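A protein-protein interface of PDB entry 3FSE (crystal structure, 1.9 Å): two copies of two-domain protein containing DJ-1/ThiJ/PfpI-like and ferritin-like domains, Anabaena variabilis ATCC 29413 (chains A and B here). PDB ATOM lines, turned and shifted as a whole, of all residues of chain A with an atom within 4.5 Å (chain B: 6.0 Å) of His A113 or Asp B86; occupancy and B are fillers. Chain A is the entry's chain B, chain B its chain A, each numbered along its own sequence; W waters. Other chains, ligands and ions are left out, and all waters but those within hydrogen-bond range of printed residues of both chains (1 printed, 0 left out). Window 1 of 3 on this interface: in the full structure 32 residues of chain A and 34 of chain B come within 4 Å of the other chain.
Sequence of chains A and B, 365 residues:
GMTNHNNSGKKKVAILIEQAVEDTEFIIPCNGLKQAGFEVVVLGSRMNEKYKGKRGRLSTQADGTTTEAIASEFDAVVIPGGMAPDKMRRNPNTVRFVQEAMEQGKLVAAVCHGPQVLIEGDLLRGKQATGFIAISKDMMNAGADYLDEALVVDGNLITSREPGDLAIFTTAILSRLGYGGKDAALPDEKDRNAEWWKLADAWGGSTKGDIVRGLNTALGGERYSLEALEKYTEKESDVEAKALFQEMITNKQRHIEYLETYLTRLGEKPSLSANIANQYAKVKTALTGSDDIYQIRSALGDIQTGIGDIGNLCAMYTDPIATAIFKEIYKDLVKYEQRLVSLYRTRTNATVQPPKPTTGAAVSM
The side-chain carboxylate (OD2) of Asp B86 is in salt-bridge range of the guanidinium group (NH2) of Arg B90, at 3.3 Å.
ND1 of His A113 lies close to SG of CSX A112 (3.7 Å).
N of Phe A132 sits at hydrogen-bond distance from O of CSX A112 (2.9 Å).
Among the printed residues, pairs that only touch across the chains: Phe A132 with Arg B90 (3.6 Å), Ala A134 with Asp B86 (3.4 Å) and Ala A134 with Arg B90 (3.8 Å).
Met B83 touches its own counterpart, Met A83.
Positions printed for both chains: 82, 83, 85 and 116.
Printed residues of chain B within 4 Å of Met A83: Met B83 (3.3 Å).
His A113 touches just one residue of chain B: Asp B86 (2.8 Å).
Gln A116 touches none of the printed residues of chain B.
Printed residues of chain B within 4 Å of Phe A132: Arg B90.
Printed residues of chain B within 4 Å of Ala A134: Asp B86, Arg B89 and Arg B90.
Of the printed residues of chain A, Met B83 touches Met A83.
Lys B87 touches none of the printed residues of chain A.
Printed residues of chain A within 4 Å of Arg B89: Ala A134 (3.0 Å).
The nearest printed residue of chain B that does not touch His A113 is Arg B90 (6.1 Å).
The nearest printed residue of chain A that does not touch Asp B86 is Met A83 (4.2 Å).
The side-chain carboxylate (OD1) of Asp B86 lies within hydrogen-bond range of a ring nitrogen (NE2) of His A113, at 2.8 Å.
NE of Arg B89 lies within hydrogen-bond range of O of Ala A134, at 3.0 Å.
The side-chain sulfur (SD) of Met B83 lies close to the side-chain sulfur (SD) of Met A83 (3.3 Å).
Of the 10 printed residues of chain B, 4 touch a printed residue of chain A.
Printed residues of chain B that touch a printed residue of chain A: Met B83, Asp B86, Arg B89 and Arg B90.
Of the 13 printed residues of chain A, 4 touch a printed residue of chain B.
Printed residues of chain A that touch a printed residue of chain B: Met A83, His A113, Phe A132 and Ala A134.
Hydrophobic or aromatic side chains of chain A within 4 Å of the printed part of chain B: Met A83, His A113, Phe A132 and Ala A134.
Along chain A the printed residues that touch a printed residue of chain B span positions 83 to 134.
Among the printed residues, 6 pairs touch across the chains.
Water W1 bridges NE2 of Gln A116 (3.3 Å) and NE2 of Gln B116 (3.3 Å).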
ATOM      1  N   GLY A  81     -25.965   3.897 -27.039  1.00  0.00           N
ATOM      2  CA  GLY A  81     -24.576   3.605 -26.790  1.00  0.00           C
ATOM      3  C   GLY A  81     -23.741   4.720 -26.245  1.00  0.00           C
ATOM      4  O   GLY A  81     -24.167   5.485 -25.360  1.00  0.00           O
ATOM      5  N   GLY A  82     -22.545   4.838 -26.806  1.00  0.00           N
ATOM      6  CA  GLY A  82     -21.539   5.734 -26.277  1.00  0.00           C
ATOM      7  C   GLY A  82     -20.941   5.028 -25.072  1.00  0.00           C
ATOM      8  O   GLY A  82     -20.846   3.796 -25.057  1.00  0.00           O
ATOM      9  N   MET A  83     -20.505   5.825 -24.109  1.00  0.00           N
ATOM     10  CA  MET A  83     -19.931   5.284 -22.887  1.00  0.00           C
ATOM     11  C   MET A  83     -21.004   5.072 -21.805  1.00  0.00           C
ATOM     12  O   MET A  83     -20.697   4.503 -20.764  1.00  0.00           O
ATOM     13  CB  MET A  83     -18.729   6.121 -22.416  1.00  0.00           C
ATOM     14  CG  MET A  83     -17.582   6.232 -23.462  1.00  0.00           C
ATOM     15  SD  MET A  83     -16.604   4.593 -24.013  1.00  0.00           S
ATOM     16  CE  MET A  83     -17.757   3.805 -25.252  1.00  0.00           C
ATOM     17  N   PRO A  85     -23.534   2.738 -21.630  1.00  0.00           N
ATOM     18  CA  PRO A  85     -23.681   1.311 -21.241  1.00  0.00           C
ATOM     19  C   PRO A  85     -22.667   0.820 -20.195  1.00  0.00           C
ATOM     20  O   PRO A  85     -23.028  -0.009 -19.372  1.00  0.00           O
ATOM     21  CB  PRO A  85     -23.557   0.576 -22.570  1.00  0.00           C
ATOM     22  CG  PRO A  85     -24.158   1.572 -23.555  1.00  0.00           C
ATOM     23  CD  PRO A  85     -23.439   2.839 -23.099  1.00  0.00           C
ATOM     24  N   VAL A 111     -28.186  -0.187 -29.700  1.00  0.00           N
ATOM     25  CA  VAL A 111     -27.297   0.279 -30.779  1.00  0.00           C
ATOM     26  C   VAL A 111     -25.914   0.570 -30.229  1.00  0.00           C
ATOM     27  O   VAL A 111     -25.796   0.980 -29.070  1.00  0.00           O
ATOM     28  CB  VAL A 111     -27.872   1.543 -31.488  1.00  0.00           C
ATOM     29  CG1 VAL A 111     -28.158   2.685 -30.469  1.00  0.00           C
ATOM     30  CG2 VAL A 111     -26.944   2.033 -32.643  1.00  0.00           C
ATOM     31  N   CSX A 112     -24.871   0.276 -31.027  1.00  0.00           N
ATOM     32  CA  CSX A 112     -23.478   0.690 -30.694  1.00  0.00           C
ATOM     33  CB  CSX A 112     -23.530   2.237 -30.678  1.00  0.00           C
ATOM     34  SG  CSX A 112     -21.970   3.173 -30.563  1.00  0.00           S
ATOM     35  C   CSX A 112     -22.926  -0.074 -29.513  1.00  0.00           C
ATOM     36  O   CSX A 112     -22.706  -1.272 -29.636  1.00  0.00           O
ATOM     37  OD  CSX A 112     -21.300   2.928 -32.133  1.00  0.00           O
ATOM     38  N   HIS A 113     -22.689   0.591 -28.375  1.00  0.00           N
ATOM     39  CA  HIS A 113     -22.234  -0.060 -27.134  1.00  0.00           C
ATOM     40  C   HIS A 113     -23.411  -0.553 -26.296  1.00  0.00           C
ATOM     41  O   HIS A 113     -23.207  -1.283 -25.302  1.00  0.00           O
ATOM     42  CB  HIS A 113     -21.345   0.832 -26.281  1.00  0.00           C
ATOM     43  CG  HIS A 113     -19.969   1.031 -26.827  1.00  0.00           C
ATOM     44  ND1 HIS A 113     -19.713   1.814 -27.935  1.00  0.00           N
ATOM     45  CD2 HIS A 113     -18.765   0.575 -26.400  1.00  0.00           C
ATOM     46  CE1 HIS A 113     -18.411   1.823 -28.165  1.00  0.00           C
ATOM     47  NE2 HIS A 113     -17.814   1.088 -27.246  1.00  0.00           N
ATOM     48  N   GLY A 114     -24.638  -0.193 -26.687  1.00  0.00           N
ATOM     49  CA  GLY A 114     -25.857  -0.656 -26.003  1.00  0.00           C
ATOM     50  C   GLY A 114     -25.885  -2.136 -25.652  1.00  0.00           C
ATOM     51  O   GLY A 114     -26.303  -2.493 -24.518  1.00  0.00           O
ATOM     52  N   PRO A 115     -25.457  -3.022 -26.582  1.00  0.00           N
ATOM     53  CA  PRO A 115     -25.404  -4.444 -26.220  1.00  0.00           C
ATOM     54  C   PRO A 115     -24.581  -4.840 -24.990  1.00  0.00           C
ATOM     55  O   PRO A 115     -24.757  -5.942 -24.525  1.00  0.00           O
ATOM     56  CB  PRO A 115     -24.911  -5.116 -27.507  1.00  0.00           C
ATOM     57  CG  PRO A 115     -25.436  -4.204 -28.574  1.00  0.00           C
ATOM     58  CD  PRO A 115     -25.124  -2.875 -28.016  1.00  0.00           C
ATOM     59  N   GLN A 116     -23.740  -3.952 -24.443  1.00  0.00           N
ATOM     60  CA  GLN A 116     -23.044  -4.235 -23.188  1.00  0.00           C
ATOM     61  C   GLN A 116     -24.024  -4.503 -22.032  1.00  0.00           C
ATOM     62  O   GLN A 116     -23.715  -5.273 -21.146  1.00  0.00           O
ATOM     63  CB  GLN A 116     -22.086  -3.110 -22.809  1.00  0.00           C
ATOM     64  CG  GLN A 116     -20.896  -3.065 -23.697  1.00  0.00           C
ATOM     65  CD  GLN A 116     -19.959  -1.938 -23.369  1.00  0.00           C
ATOM     66  OE1 GLN A 116     -20.381  -0.799 -23.144  1.00  0.00           O
ATOM     67  NE2 GLN A 116     -18.680  -2.238 -23.373  1.00  0.00           N
ATOM     68  N   PHE A 132     -21.325  -2.118 -31.993  1.00  0.00           N
ATOM     69  CA  PHE A 132     -20.119  -1.408 -32.418  1.00  0.00           C
ATOM     70  C   PHE A 132     -18.957  -2.390 -32.461  1.00  0.00           C
ATOM     71  O   PHE A 132     -18.842  -3.287 -31.600  1.00  0.00           O
ATOM     72  CB  PHE A 132     -19.811  -0.201 -31.543  1.00  0.00           C
ATOM     73  CG  PHE A 132     -18.727   0.680 -32.102  1.00  0.00           C
ATOM     74  CD1 PHE A 132     -18.878   1.284 -33.361  1.00  0.00           C
ATOM     75  CD2 PHE A 132     -17.581   0.933 -31.382  1.00  0.00           C
ATOM     76  CE1 PHE A 132     -17.869   2.104 -33.899  1.00  0.00           C
ATOM     77  CE2 PHE A 132     -16.576   1.772 -31.898  1.00  0.00           C
ATOM     78  CZ  PHE A 132     -16.726   2.349 -33.172  1.00  0.00           C
ATOM     79  N   ALA A 134     -15.939  -2.257 -31.752  1.00  0.00           N
ATOM     80  CA  ALA A 134     -15.096  -2.270 -30.539  1.00  0.00           C
ATOM     81  C   ALA A 134     -15.544  -3.333 -29.527  1.00  0.00           C
ATOM     82  O   ALA A 134     -14.702  -3.868 -28.829  1.00  0.00           O
ATOM     83  CB  ALA A 134     -15.049  -0.848 -29.854  1.00  0.00           C
ATOM     84  N   ILE A 135     -16.849  -3.649 -29.477  1.00  0.00           N
ATOM     85  CA  ILE A 135     -17.381  -4.664 -28.542  1.00  0.00           C
ATOM     86  C   ILE A 135     -17.725  -6.007 -29.194  1.00  0.00           C
ATOM     87  O   ILE A 135     -18.268  -6.871 -28.528  1.00  0.00           O
ATOM     88  CB  ILE A 135     -18.591  -4.145 -27.705  1.00  0.00           C
ATOM     89  CG1 ILE A 135     -19.861  -3.915 -28.540  1.00  0.00           C
ATOM     90  CG2 ILE A 135     -18.227  -2.859 -26.954  1.00  0.00           C
ATOM     91  CD1 ILE A 135     -21.107  -3.763 -27.664  1.00  0.00           C
ATOM     92  N   GLY B  82      -9.472   3.756 -18.320  1.00  0.00           N
ATOM     93  CA  GLY B  82     -10.374   4.831 -18.717  1.00  0.00           C
ATOM     94  C   GLY B  82     -11.037   4.328 -19.990  1.00  0.00           C
ATOM     95  O   GLY B  82     -11.240   3.117 -20.132  1.00  0.00           O
ATOM     96  N   MET B  83     -11.345   5.251 -20.898  1.00  0.00           N
ATOM     97  CA  MET B  83     -11.963   4.886 -22.170  1.00  0.00           C
ATOM     98  C   MET B  83     -10.929   4.635 -23.278  1.00  0.00           C
ATOM     99  O   MET B  83     -11.297   4.250 -24.388  1.00  0.00           O
ATOM    100  CB  MET B  83     -13.034   5.912 -22.592  1.00  0.00           C
ATOM    101  CG  MET B  83     -14.238   6.024 -21.622  1.00  0.00           C
ATOM    102  SD  MET B  83     -15.214   4.379 -21.018  1.00  0.00           S
ATOM    103  CE  MET B  83     -14.236   3.947 -19.382  1.00  0.00           C
ATOM    104  N   ALA B  84      -9.632   4.787 -22.972  1.00  0.00           N
ATOM    105  CA  ALA B  84      -8.571   4.540 -23.954  1.00  0.00           C
ATOM    106  C   ALA B  84      -8.570   3.117 -24.569  1.00  0.00           C
ATOM    107  O   ALA B  84      -8.373   2.977 -25.782  1.00  0.00           O
ATOM    108  CB  ALA B  84      -7.168   4.887 -23.359  1.00  0.00           C
ATOM    109  N   PRO B  85      -8.735   2.058 -23.745  1.00  0.00           N
ATOM    110  CA  PRO B  85      -8.774   0.689 -24.335  1.00  0.00           C
ATOM    111  C   PRO B  85      -9.837   0.445 -25.422  1.00  0.00           C
ATOM    112  O   PRO B  85      -9.593  -0.338 -26.327  1.00  0.00           O
ATOM    113  CB  PRO B  85      -8.999  -0.204 -23.111  1.00  0.00           C
ATOM    114  CG  PRO B  85      -8.350   0.544 -22.018  1.00  0.00           C
ATOM    115  CD  PRO B  85      -8.763   1.988 -22.276  1.00  0.00           C
ATOM    116  N   ASP B  86     -10.964   1.169 -25.370  1.00  0.00           N
ATOM    117  CA  ASP B  86     -12.012   1.062 -26.382  1.00  0.00           C
ATOM    118  C   ASP B  86     -11.445   1.476 -27.764  1.00  0.00           C
ATOM    119  O   ASP B  86     -11.830   0.931 -28.770  1.00  0.00           O
ATOM    120  CB  ASP B  86     -13.221   1.912 -26.000  1.00  0.00           C
ATOM    121  CG  ASP B  86     -14.408   1.707 -26.939  1.00  0.00           C
ATOM    122  OD1 ASP B  86     -15.114   0.695 -26.799  1.00  0.00           O
ATOM    123  OD2 ASP B  86     -14.642   2.579 -27.792  1.00  0.00           O
ATOM    124  N   LYS B  87     -10.465   2.377 -27.780  1.00  0.00           N
ATOM    125  CA  LYS B  87      -9.826   2.819 -29.018  1.00  0.00           C
ATOM    126  C   LYS B  87      -8.588   1.933 -29.291  1.00  0.00           C
ATOM    127  O   LYS B  87      -8.346   1.585 -30.424  1.00  0.00           O
ATOM    128  CB  LYS B  87      -9.473   4.289 -28.895  1.00  0.00           C
ATOM    129  CG  LYS B  87      -8.887   4.944 -30.111  1.00  0.00           C
ATOM    130  CD  LYS B  87      -9.832   5.119 -31.285  1.00  0.00           C
ATOM    131  CE  LYS B  87      -9.143   5.959 -32.385  1.00  0.00           C
ATOM    132  NZ  LYS B  87      -7.616   5.742 -32.626  1.00  0.00           N
ATOM    133  N   MET B  88      -7.806   1.586 -28.262  1.00  0.00           N
ATOM    134  CA  MET B  88      -6.619   0.727 -28.474  1.00  0.00           C
ATOM    135  C   MET B  88      -6.978  -0.649 -29.072  1.00  0.00           C
ATOM    136  O   MET B  88      -6.253  -1.174 -29.925  1.00  0.00           O
ATOM    137  CB  MET B  88      -5.871   0.483 -27.176  1.00  0.00           C
ATOM    138  CG  MET B  88      -5.245   1.664 -26.518  1.00  0.00           C
ATOM    139  SD  MET B  88      -4.689   1.055 -24.674  1.00  0.00           S
ATOM    140  CE  MET B  88      -4.231   2.826 -23.968  1.00  0.00           C
ATOM    141  N   ARG B  89      -8.101  -1.230 -28.619  1.00  0.00           N
ATOM    142  CA  ARG B  89      -8.516  -2.548 -29.099  1.00  0.00           C
ATOM    143  C   ARG B  89      -8.928  -2.571 -30.568  1.00  0.00           C
ATOM    144  O   ARG B  89      -8.965  -3.650 -31.189  1.00  0.00           O
ATOM    145  CB  ARG B  89      -9.612  -3.126 -28.233  1.00  0.00           C
ATOM    146  CG  ARG B  89     -10.947  -2.510 -28.429  1.00  0.00           C
ATOM    147  CD  ARG B  89     -11.921  -2.945 -27.341  1.00  0.00           C
ATOM    148  NE  ARG B  89     -12.110  -4.392 -27.312  1.00  0.00           N
ATOM    149  CZ  ARG B  89     -12.995  -5.012 -26.534  1.00  0.00           C
ATOM    150  NH1 ARG B  89     -13.754  -4.340 -25.681  1.00  0.00           N
ATOM    151  NH2 ARG B  89     -13.103  -6.312 -26.608  1.00  0.00           N
ATOM    152  N   ARG B  90      -9.268  -1.404 -31.114  1.00  0.00           N
ATOM    153  CA  ARG B  90      -9.531  -1.257 -32.562  1.00  0.00           C
ATOM    154  C   ARG B  90      -8.261  -1.055 -33.421  1.00  0.00           C
ATOM    155  O   ARG B  90      -8.354  -1.030 -34.630  1.00  0.00           O
ATOM    156  CB  ARG B  90     -10.497  -0.100 -32.790  1.00  0.00           C
ATOM    157  CG  ARG B  90     -11.908  -0.396 -32.301  1.00  0.00           C
ATOM    158  CD  ARG B  90     -12.816   0.785 -32.605  1.00  0.00           C
ATOM    159  NE  ARG B  90     -12.856   1.731 -31.498  1.00  0.00           N
ATOM    160  CZ  ARG B  90     -13.142   3.033 -31.585  1.00  0.00           C
ATOM    161  NH1 ARG B  90     -13.405   3.639 -32.757  1.00  0.00           N
ATOM    162  NH2 ARG B  90     -13.143   3.748 -30.462  1.00  0.00           N
ATOM    163  N   GLN B 116      -9.364  -4.913 -21.569  1.00  0.00           N
ATOM    164  CA  GLN B 116     -10.089  -4.990 -22.850  1.00  0.00           C
ATOM    165  C   GLN B 116      -9.175  -5.287 -24.053  1.00  0.00           C
ATOM    166  O   GLN B 116      -9.594  -5.909 -25.008  1.00  0.00           O
ATOM    167  CB  GLN B 116     -10.922  -3.736 -23.116  1.00  0.00           C
ATOM    168  CG  GLN B 116     -12.103  -3.599 -22.187  1.00  0.00           C
ATOM    169  CD  GLN B 116     -12.931  -2.359 -22.442  1.00  0.00           C
ATOM    170  OE1 GLN B 116     -12.395  -1.270 -22.670  1.00  0.00           O
ATOM    171  NE2 GLN B 116     -14.249  -2.509 -22.381  1.00  0.00           N
HETATM  172  O   HOH W   1     -16.357   0.062 -22.702  1.00  0.00           O
